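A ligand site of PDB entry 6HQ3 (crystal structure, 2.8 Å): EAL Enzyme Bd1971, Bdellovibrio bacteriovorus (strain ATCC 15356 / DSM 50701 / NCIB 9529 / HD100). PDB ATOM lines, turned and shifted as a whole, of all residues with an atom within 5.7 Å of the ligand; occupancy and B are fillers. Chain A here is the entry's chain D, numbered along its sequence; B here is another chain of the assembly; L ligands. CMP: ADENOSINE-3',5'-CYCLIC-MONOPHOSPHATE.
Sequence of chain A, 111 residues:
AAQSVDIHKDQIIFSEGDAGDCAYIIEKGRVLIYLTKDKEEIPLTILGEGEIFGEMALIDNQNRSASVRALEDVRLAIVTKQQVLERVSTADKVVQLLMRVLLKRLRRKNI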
ATOM      1  N   PHE A  14      22.110   0.831  17.038  1.00  0.00           N
ATOM      2  CA  PHE A  14      21.015  -0.134  17.005  1.00  0.00           C
ATOM      3  C   PHE A  14      20.468  -0.342  18.413  1.00  0.00           C
ATOM      4  O   PHE A  14      21.060   0.129  19.393  1.00  0.00           O
ATOM      5  CB  PHE A  14      21.431  -1.477  16.341  1.00  0.00           C
ATOM      6  CG  PHE A  14      22.609  -2.179  16.997  1.00  0.00           C
ATOM      7  CD1 PHE A  14      22.455  -2.857  18.215  1.00  0.00           C
ATOM      8  CD2 PHE A  14      23.853  -2.221  16.365  1.00  0.00           C
ATOM      9  CE1 PHE A  14      23.524  -3.526  18.788  1.00  0.00           C
ATOM     10  CE2 PHE A  14      24.933  -2.889  16.946  1.00  0.00           C
ATOM     11  CZ  PHE A  14      24.755  -3.548  18.159  1.00  0.00           C
ATOM     12  N   ILE A  33      27.339   0.923  25.226  1.00  0.00           N
ATOM     13  CA  ILE A  33      26.492  -0.277  25.210  1.00  0.00           C
ATOM     14  C   ILE A  33      25.607  -0.190  26.445  1.00  0.00           C
ATOM     15  O   ILE A  33      26.115  -0.019  27.560  1.00  0.00           O
ATOM     16  CB  ILE A  33      27.315  -1.601  25.261  1.00  0.00           C
ATOM     17  CG1 ILE A  33      27.997  -1.909  23.928  1.00  0.00           C
ATOM     18  CG2 ILE A  33      26.395  -2.797  25.502  1.00  0.00           C
ATOM     19  CD1 ILE A  33      28.940  -0.851  23.421  1.00  0.00           C
ATOM     20  N   LEU A  35      21.344  -1.268  28.294  1.00  0.00           N
ATOM     21  CA  LEU A  35      19.981  -1.780  28.258  1.00  0.00           C
ATOM     22  C   LEU A  35      19.027  -0.714  28.764  1.00  0.00           C
ATOM     23  O   LEU A  35      19.429   0.196  29.489  1.00  0.00           O
ATOM     24  CB  LEU A  35      19.809  -3.021  29.139  1.00  0.00           C
ATOM     25  CG  LEU A  35      20.831  -4.147  28.984  1.00  0.00           C
ATOM     26  CD1 LEU A  35      20.596  -5.209  30.043  1.00  0.00           C
ATOM     27  CD2 LEU A  35      20.773  -4.750  27.585  1.00  0.00           C
ATOM     28  N   LEU A  44      26.249  -0.535  30.381  1.00  0.00           N
ATOM     29  CA  LEU A  44      27.006  -1.769  30.495  1.00  0.00           C
ATOM     30  C   LEU A  44      28.500  -1.524  30.311  1.00  0.00           C
ATOM     31  O   LEU A  44      29.310  -1.874  31.174  1.00  0.00           O
ATOM     32  CB  LEU A  44      26.488  -2.806  29.495  1.00  0.00           C
ATOM     33  CG  LEU A  44      25.043  -3.263  29.725  1.00  0.00           C
ATOM     34  CD1 LEU A  44      24.470  -3.930  28.470  1.00  0.00           C
ATOM     35  CD2 LEU A  44      24.959  -4.174  30.920  1.00  0.00           C
ATOM     36  N   THR A  45      28.861  -0.912  29.201  1.00  0.00           N
ATOM     37  CA  THR A  45      30.263  -0.596  28.940  1.00  0.00           C
ATOM     38  C   THR A  45      30.360   0.543  27.940  1.00  0.00           C
ATOM     39  O   THR A  45      29.383   0.885  27.287  1.00  0.00           O
ATOM     40  CB  THR A  45      31.014  -1.849  28.464  1.00  0.00           C
ATOM     41  OG1 THR A  45      32.394  -1.537  28.238  1.00  0.00           O
ATOM     42  CG2 THR A  45      30.383  -2.420  27.166  1.00  0.00           C
ATOM     43  N   LEU A  47      32.894   1.523  24.703  1.00  0.00           N
ATOM     44  CA  LEU A  47      33.968   1.061  23.805  1.00  0.00           C
ATOM     45  C   LEU A  47      34.501   2.217  23.004  1.00  0.00           C
ATOM     46  O   LEU A  47      33.755   3.158  22.691  1.00  0.00           O
ATOM     47  CB  LEU A  47      33.441   0.026  22.820  1.00  0.00           C
ATOM     48  CG  LEU A  47      32.705  -1.207  23.331  1.00  0.00           C
ATOM     49  CD1 LEU A  47      32.374  -2.098  22.138  1.00  0.00           C
ATOM     50  CD2 LEU A  47      33.487  -1.960  24.415  1.00  0.00           C
ATOM     51  N   ILE A  52      35.398  -3.750  18.793  1.00  0.00           N
ATOM     52  CA  ILE A  52      34.330  -4.348  17.982  1.00  0.00           C
ATOM     53  C   ILE A  52      33.083  -4.654  18.815  1.00  0.00           C
ATOM     54  O   ILE A  52      33.178  -5.088  19.964  1.00  0.00           O
ATOM     55  CB  ILE A  52      34.808  -5.615  17.225  1.00  0.00           C
ATOM     56  CG1 ILE A  52      33.826  -6.014  16.134  1.00  0.00           C
ATOM     57  CG2 ILE A  52      35.032  -6.788  18.162  1.00  0.00           C
ATOM     58  CD1 ILE A  52      34.328  -7.111  15.233  1.00  0.00           C
ATOM     59  N   PHE A  53      31.931  -4.414  18.212  1.00  0.00           N
ATOM     60  CA  PHE A  53      30.657  -4.778  18.819  1.00  0.00           C
ATOM     61  C   PHE A  53      29.687  -5.326  17.782  1.00  0.00           C
ATOM     62  O   PHE A  53      29.917  -5.213  16.580  1.00  0.00           O
ATOM     63  CB  PHE A  53      30.059  -3.611  19.607  1.00  0.00           C
ATOM     64  CG  PHE A  53      29.723  -2.407  18.788  1.00  0.00           C
ATOM     65  CD1 PHE A  53      28.470  -2.290  18.163  1.00  0.00           C
ATOM     66  CD2 PHE A  53      30.630  -1.350  18.652  1.00  0.00           C
ATOM     67  CE1 PHE A  53      28.146  -1.168  17.416  1.00  0.00           C
ATOM     68  CE2 PHE A  53      30.303  -0.231  17.883  1.00  0.00           C
ATOM     69  CZ  PHE A  53      29.068  -0.149  17.275  1.00  0.00           C
ATOM     70  N   GLY A  54      28.605  -5.909  18.279  1.00  0.00           N
ATOM     71  CA  GLY A  54      27.550  -6.426  17.424  1.00  0.00           C
ATOM     72  C   GLY A  54      27.883  -7.763  16.810  1.00  0.00           C
ATOM     73  O   GLY A  54      27.336  -8.152  15.787  1.00  0.00           O
ATOM     74  N   GLU A  55      28.757  -8.508  17.474  1.00  0.00           N
ATOM     75  CA  GLU A  55      29.085  -9.855  17.065  1.00  0.00           C
ATOM     76  C   GLU A  55      28.005 -10.890  17.480  1.00  0.00           C
ATOM     77  O   GLU A  55      27.873 -11.885  16.804  1.00  0.00           O
ATOM     78  CB  GLU A  55      30.486 -10.239  17.564  1.00  0.00           C
ATOM     79  CG  GLU A  55      30.647 -10.541  19.051  1.00  0.00           C
ATOM     80  CD  GLU A  55      30.854  -9.325  19.930  1.00  0.00           C
ATOM     81  OE1 GLU A  55      30.870  -8.159  19.435  1.00  0.00           O
ATOM     82  OE2 GLU A  55      31.093  -9.520  21.136  1.00  0.00           O
ATOM     83  N   MET A  56      27.305 -10.645  18.587  1.00  0.00           N
ATOM     84  CA  MET A  56      26.564 -11.755  19.219  1.00  0.00           C
ATOM     85  C   MET A  56      25.372 -12.236  18.389  1.00  0.00           C
ATOM     86  O   MET A  56      25.109 -13.446  18.292  1.00  0.00           O
ATOM     87  CB  MET A  56      26.113 -11.434  20.638  1.00  0.00           C
ATOM     88  CG  MET A  56      27.258 -11.295  21.619  1.00  0.00           C
ATOM     89  SD  MET A  56      28.448 -12.663  21.721  1.00  0.00           S
ATOM     90  CE  MET A  56      27.571 -13.959  22.606  1.00  0.00           C
ATOM     91  N   ALA A  57      24.694 -11.279  17.758  1.00  0.00           N
ATOM     92  CA  ALA A  57      23.656 -11.596  16.794  1.00  0.00           C
ATOM     93  C   ALA A  57      24.153 -12.484  15.662  1.00  0.00           C
ATOM     94  O   ALA A  57      23.425 -13.285  15.127  1.00  0.00           O
ATOM     95  CB  ALA A  57      23.088 -10.324  16.195  1.00  0.00           C
ATOM     96  N   LEU A  58      25.415 -12.271  15.281  1.00  0.00           N
ATOM     97  CA  LEU A  58      26.038 -12.978  14.175  1.00  0.00           C
ATOM     98  C   LEU A  58      26.389 -14.412  14.519  1.00  0.00           C
ATOM     99  O   LEU A  58      25.927 -15.338  13.862  1.00  0.00           O
ATOM    100  CB  LEU A  58      27.258 -12.188  13.708  1.00  0.00           C
ATOM    101  CG  LEU A  58      26.963 -10.938  12.833  1.00  0.00           C
ATOM    102  CD1 LEU A  58      25.844 -10.017  13.339  1.00  0.00           C
ATOM    103  CD2 LEU A  58      28.282 -10.155  12.647  1.00  0.00           C
ATOM    104  N   ASN A  63      18.695 -11.884  17.804  1.00  0.00           N
ATOM    105  CA  ASN A  63      18.629 -10.419  17.801  1.00  0.00           C
ATOM    106  C   ASN A  63      19.710  -9.747  18.645  1.00  0.00           C
ATOM    107  O   ASN A  63      20.528 -10.395  19.302  1.00  0.00           O
ATOM    108  CB  ASN A  63      17.227 -10.027  18.286  1.00  0.00           C
ATOM    109  CG  ASN A  63      16.134 -10.364  17.267  1.00  0.00           C
ATOM    110  OD1 ASN A  63      16.422 -10.613  16.092  1.00  0.00           O
ATOM    111  ND2 ASN A  63      14.896 -10.338  17.709  1.00  0.00           N
ATOM    112  N   ARG A  64      19.694  -8.413  18.621  1.00  0.00           N
ATOM    113  CA  ARG A  64      20.625  -7.601  19.378  1.00  0.00           C
ATOM    114  C   ARG A  64      20.304  -7.729  20.855  1.00  0.00           C
ATOM    115  O   ARG A  64      19.145  -7.521  21.265  1.00  0.00           O
ATOM    116  CB  ARG A  64      20.556  -6.117  18.954  1.00  0.00           C
ATOM    117  CG  ARG A  64      20.881  -5.836  17.488  1.00  0.00           C
ATOM    118  CD  ARG A  64      22.254  -6.351  17.104  1.00  0.00           C
ATOM    119  NE  ARG A  64      22.696  -5.852  15.791  1.00  0.00           N
ATOM    120  CZ  ARG A  64      23.894  -6.055  15.254  1.00  0.00           C
ATOM    121  NH1 ARG A  64      24.786  -6.780  15.885  1.00  0.00           N
ATOM    122  NH2 ARG A  64      24.200  -5.553  14.060  1.00  0.00           N
ATOM    123  N   SER A  65      21.315  -8.108  21.632  1.00  0.00           N
ATOM    124  CA  SER A  65      21.162  -8.321  23.070  1.00  0.00           C
ATOM    125  C   SER A  65      21.187  -7.017  23.881  1.00  0.00           C
ATOM    126  O   SER A  65      20.703  -6.979  25.023  1.00  0.00           O
ATOM    127  CB  SER A  65      22.241  -9.250  23.572  1.00  0.00           C
ATOM    128  OG  SER A  65      23.495  -8.743  23.239  1.00  0.00           O
ATOM    129  N   ALA A  66      21.734  -5.952  23.294  1.00  0.00           N
ATOM    130  CA  ALA A  66      21.828  -4.646  23.956  1.00  0.00           C
ATOM    131  C   ALA A  66      21.646  -3.544  22.951  1.00  0.00           C
ATOM    132  O   ALA A  66      21.705  -3.786  21.751  1.00  0.00           O
ATOM    133  CB  ALA A  66      23.161  -4.497  24.655  1.00  0.00           C
ATOM    134  N   SER A  67      21.411  -2.343  23.459  1.00  0.00           N
ATOM    135  CA  SER A  67      21.350  -1.138  22.631  1.00  0.00           C
ATOM    136  C   SER A  67      22.730  -0.507  22.608  1.00  0.00           C
ATOM    137  O   SER A  67      23.549  -0.721  23.530  1.00  0.00           O
ATOM    138  CB  SER A  67      20.326  -0.158  23.179  1.00  0.00           C
ATOM    139  OG  SER A  67      19.019  -0.716  23.129  1.00  0.00           O
ATOM    140  N   VAL A  68      22.994   0.251  21.549  1.00  0.00           N
ATOM    141  CA  VAL A  68      24.256   0.953  21.385  1.00  0.00           C
ATOM    142  C   VAL A  68      24.012   2.375  20.875  1.00  0.00           C
ATOM    143  O   VAL A  68      23.292   2.570  19.895  1.00  0.00           O
ATOM    144  CB  VAL A  68      25.193   0.221  20.410  1.00  0.00           C
ATOM    145  CG1 VAL A  68      26.494   0.983  20.257  1.00  0.00           C
ATOM    146  CG2 VAL A  68      25.455  -1.207  20.905  1.00  0.00           C
ATOM    147  N   VAL B 101      37.376  -8.453  23.194  1.00  0.00           N
ATOM    148  CA  VAL B 101      36.110  -8.018  23.804  1.00  0.00           C
ATOM    149  C   VAL B 101      35.412  -9.123  24.567  1.00  0.00           C
ATOM    150  O   VAL B 101      34.703  -8.859  25.541  1.00  0.00           O
ATOM    151  CB  VAL B 101      35.123  -7.387  22.782  1.00  0.00           C
ATOM    152  CG1 VAL B 101      34.478  -8.483  21.963  1.00  0.00           C
ATOM    153  CG2 VAL B 101      34.100  -6.517  23.462  1.00  0.00           C
ATOM    154  N   LYS B 104      37.460  -9.073  27.868  1.00  0.00           N
ATOM    155  CA  LYS B 104      37.012  -7.884  28.591  1.00  0.00           C
ATOM    156  C   LYS B 104      35.618  -8.074  29.189  1.00  0.00           C
ATOM    157  O   LYS B 104      35.365  -7.644  30.322  1.00  0.00           O
ATOM    158  CB  LYS B 104      37.052  -6.661  27.668  1.00  0.00           C
ATOM    159  CG  LYS B 104      36.581  -5.339  28.277  1.00  0.00           C
ATOM    160  CD  LYS B 104      35.119  -4.988  27.944  1.00  0.00           C
ATOM    161  CE  LYS B 104      34.803  -4.786  26.451  1.00  0.00           C
ATOM    162  NZ  LYS B 104      33.372  -5.153  26.172  1.00  0.00           N
ATOM    163  N   ARG B 105      34.718  -8.719  28.439  1.00  0.00           N
ATOM    164  CA  ARG B 105      33.362  -8.985  28.924  1.00  0.00           C
ATOM    165  C   ARG B 105      33.343  -9.989  30.070  1.00  0.00           C
ATOM    166  O   ARG B 105      32.585  -9.809  31.029  1.00  0.00           O
ATOM    167  CB  ARG B 105      32.457  -9.499  27.794  1.00  0.00           C
ATOM    168  CG  ARG B 105      30.979  -9.255  28.066  1.00  0.00           C
ATOM    169  CD  ARG B 105      30.144  -9.656  26.878  1.00  0.00           C
ATOM    170  NE  ARG B 105      30.472  -8.819  25.733  1.00  0.00           N
ATOM    171  CZ  ARG B 105      30.432  -9.200  24.458  1.00  0.00           C
ATOM    172  NH1 ARG B 105      30.079 -10.434  24.110  1.00  0.00           N
ATOM    173  NH2 ARG B 105      30.752  -8.329  23.504  1.00  0.00           N
ATOM    174  N   ARG B 108      34.346  -8.309  33.372  1.00  0.00           N
ATOM    175  CA  ARG B 108      33.211  -7.551  33.902  1.00  0.00           C
ATOM    176  C   ARG B 108      32.108  -8.459  34.466  1.00  0.00           C
ATOM    177  O   ARG B 108      31.437  -8.082  35.417  1.00  0.00           O
ATOM    178  CB  ARG B 108      32.614  -6.631  32.822  1.00  0.00           C
ATOM    179  CG  ARG B 108      33.480  -5.441  32.442  1.00  0.00           C
ATOM    180  CD  ARG B 108      32.703  -4.414  31.627  1.00  0.00           C
ATOM    181  NE  ARG B 108      32.355  -4.910  30.283  1.00  0.00           N
ATOM    182  CZ  ARG B 108      31.130  -5.190  29.829  1.00  0.00           C
ATOM    183  NH1 ARG B 108      30.027  -5.018  30.564  1.00  0.00           N
ATOM    184  NH2 ARG B 108      30.982  -5.646  28.590  1.00  0.00           N
HETATM  185  P   CMP L   1      24.876  -7.930  19.748  1.00  0.00           P
HETATM  186  O1P CMP L   1      24.812  -8.271  18.307  1.00  0.00           O
HETATM  187  O2P CMP L   1      23.918  -8.926  20.293  1.00  0.00           O
HETATM  188  O5' CMP L   1      24.214  -6.395  20.137  1.00  0.00           O
HETATM  189  C5' CMP L   1      24.727  -5.738  21.382  1.00  0.00           C
HETATM  190  C4' CMP L   1      26.169  -5.873  21.349  1.00  0.00           C
HETATM  191  O4' CMP L   1      26.763  -5.169  22.474  1.00  0.00           O
HETATM  192  C3' CMP L   1      26.593  -7.313  21.486  1.00  0.00           C
HETATM  193  O3' CMP L   1      26.381  -8.041  20.308  1.00  0.00           O
HETATM  194  C2' CMP L   1      27.968  -7.243  21.987  1.00  0.00           C
HETATM  195  O2' CMP L   1      28.940  -7.233  20.957  1.00  0.00           O
HETATM  196  C1' CMP L   1      28.072  -5.928  22.751  1.00  0.00           C
HETATM  197  N9  CMP L   1      28.222  -6.065  24.087  1.00  0.00           N
HETATM  198  C8  CMP L   1      29.352  -5.698  24.703  1.00  0.00           C
HETATM  199  N7  CMP L   1      29.180  -5.941  26.042  1.00  0.00           N
HETATM  200  C5  CMP L   1      27.829  -6.476  26.204  1.00  0.00           C
HETATM  201  C6  CMP L   1      27.105  -6.893  27.287  1.00  0.00           C
HETATM  202  N6  CMP L   1      27.718  -6.826  28.581  1.00  0.00           N
HETATM  203  N1  CMP L   1      25.823  -7.359  27.146  1.00  0.00           N
HETATM  204  C2  CMP L   1      25.227  -7.415  25.876  1.00  0.00           C
HETATM  205  N3  CMP L   1      26.000  -6.987  24.781  1.00  0.00           N
HETATM  206  C4  CMP L   1      27.257  -6.527  24.935  1.00  0.00           C
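Phe 14 touches the ligand (CE1 to O5', 3.2 Å). Ile 33 touches the ligand (CG1 to O4', 3.8 Å). CD1 of Leu 44 touches N1 of the ligand, at 3.9 Å. Thr 45 touches the ligand (CG2 to N7, 3.9 Å). CA of Phe 53 touches O2' of the ligand, 3.7 Å away. O of Asn 63 touches O2P of the ligand, at 3.8 Å. Ala 66 touches the ligand. Hydrophobic or aromatic side chains within 4 Å of the ligand: Phe 14, Ile 33, Leu 44, Met 56, Ala 57 and Ala 66. Along chain A the residues within 4 Å of the ligand span positions 14 to 66.
The side-chain carboxylate of Glu 55 lies within hydrogen-bond range of an oxygen (O2') of the ligand, 2.6 Å away. NH1 of Arg 64 lies within salt-bridge range of O1P of the ligand. O2P of the ligand lies within hydrogen-bond range of N of Ser 65. OG of Ser 65 lies within hydrogen-bond range of O2P of the ligand. The backbone NH (N) of Gly 54 is in hydrogen-bond range of an oxygen (O2') of the ligand, at 3.0 Å. O1P of the ligand is in hydrogen-bond range of N of Ala 57, 3.1 Å away. NH2 of Arg 108 of chain B is in hydrogen-bond range of N7 of the ligand. NE of Arg 105 of chain B is in hydrogen-bond range of N7 of the ligand (3.2 Å). N of Met 56 is in hydrogen-bond range of O3' of the ligand, 3.3 Å away.
The side-chain carboxylate (OE2) of Glu 55 lies within salt-bridge range of the guanidinium group (NH2) of Arg 105 of chain B (2.7 Å). The guanidinium group of Arg 64 is in hydrogen-bond range of the backbone carbonyl oxygen of Gly 54 (2.9 Å). NH1 of Arg 108 of chain B lies within hydrogen-bond range of O of Leu 44 (3.3 Å). The side-chain sulfur of Met 56 sits at hydrogen-bond distance from the guanidinium group of Arg 105 of chain B, at 3.7 Å. The backbone NH of Val 68 sits at hydrogen-bond distance from the backbone carbonyl oxygen of Phe 14. O of Thr 45 lies within hydrogen-bond range of N of Ile 33, at 2.9 Å. The backbone carbonyl oxygen (O) of Ile 33 is in hydrogen-bond range of the backbone NH (N) of Leu 44, 2.9 Å away.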
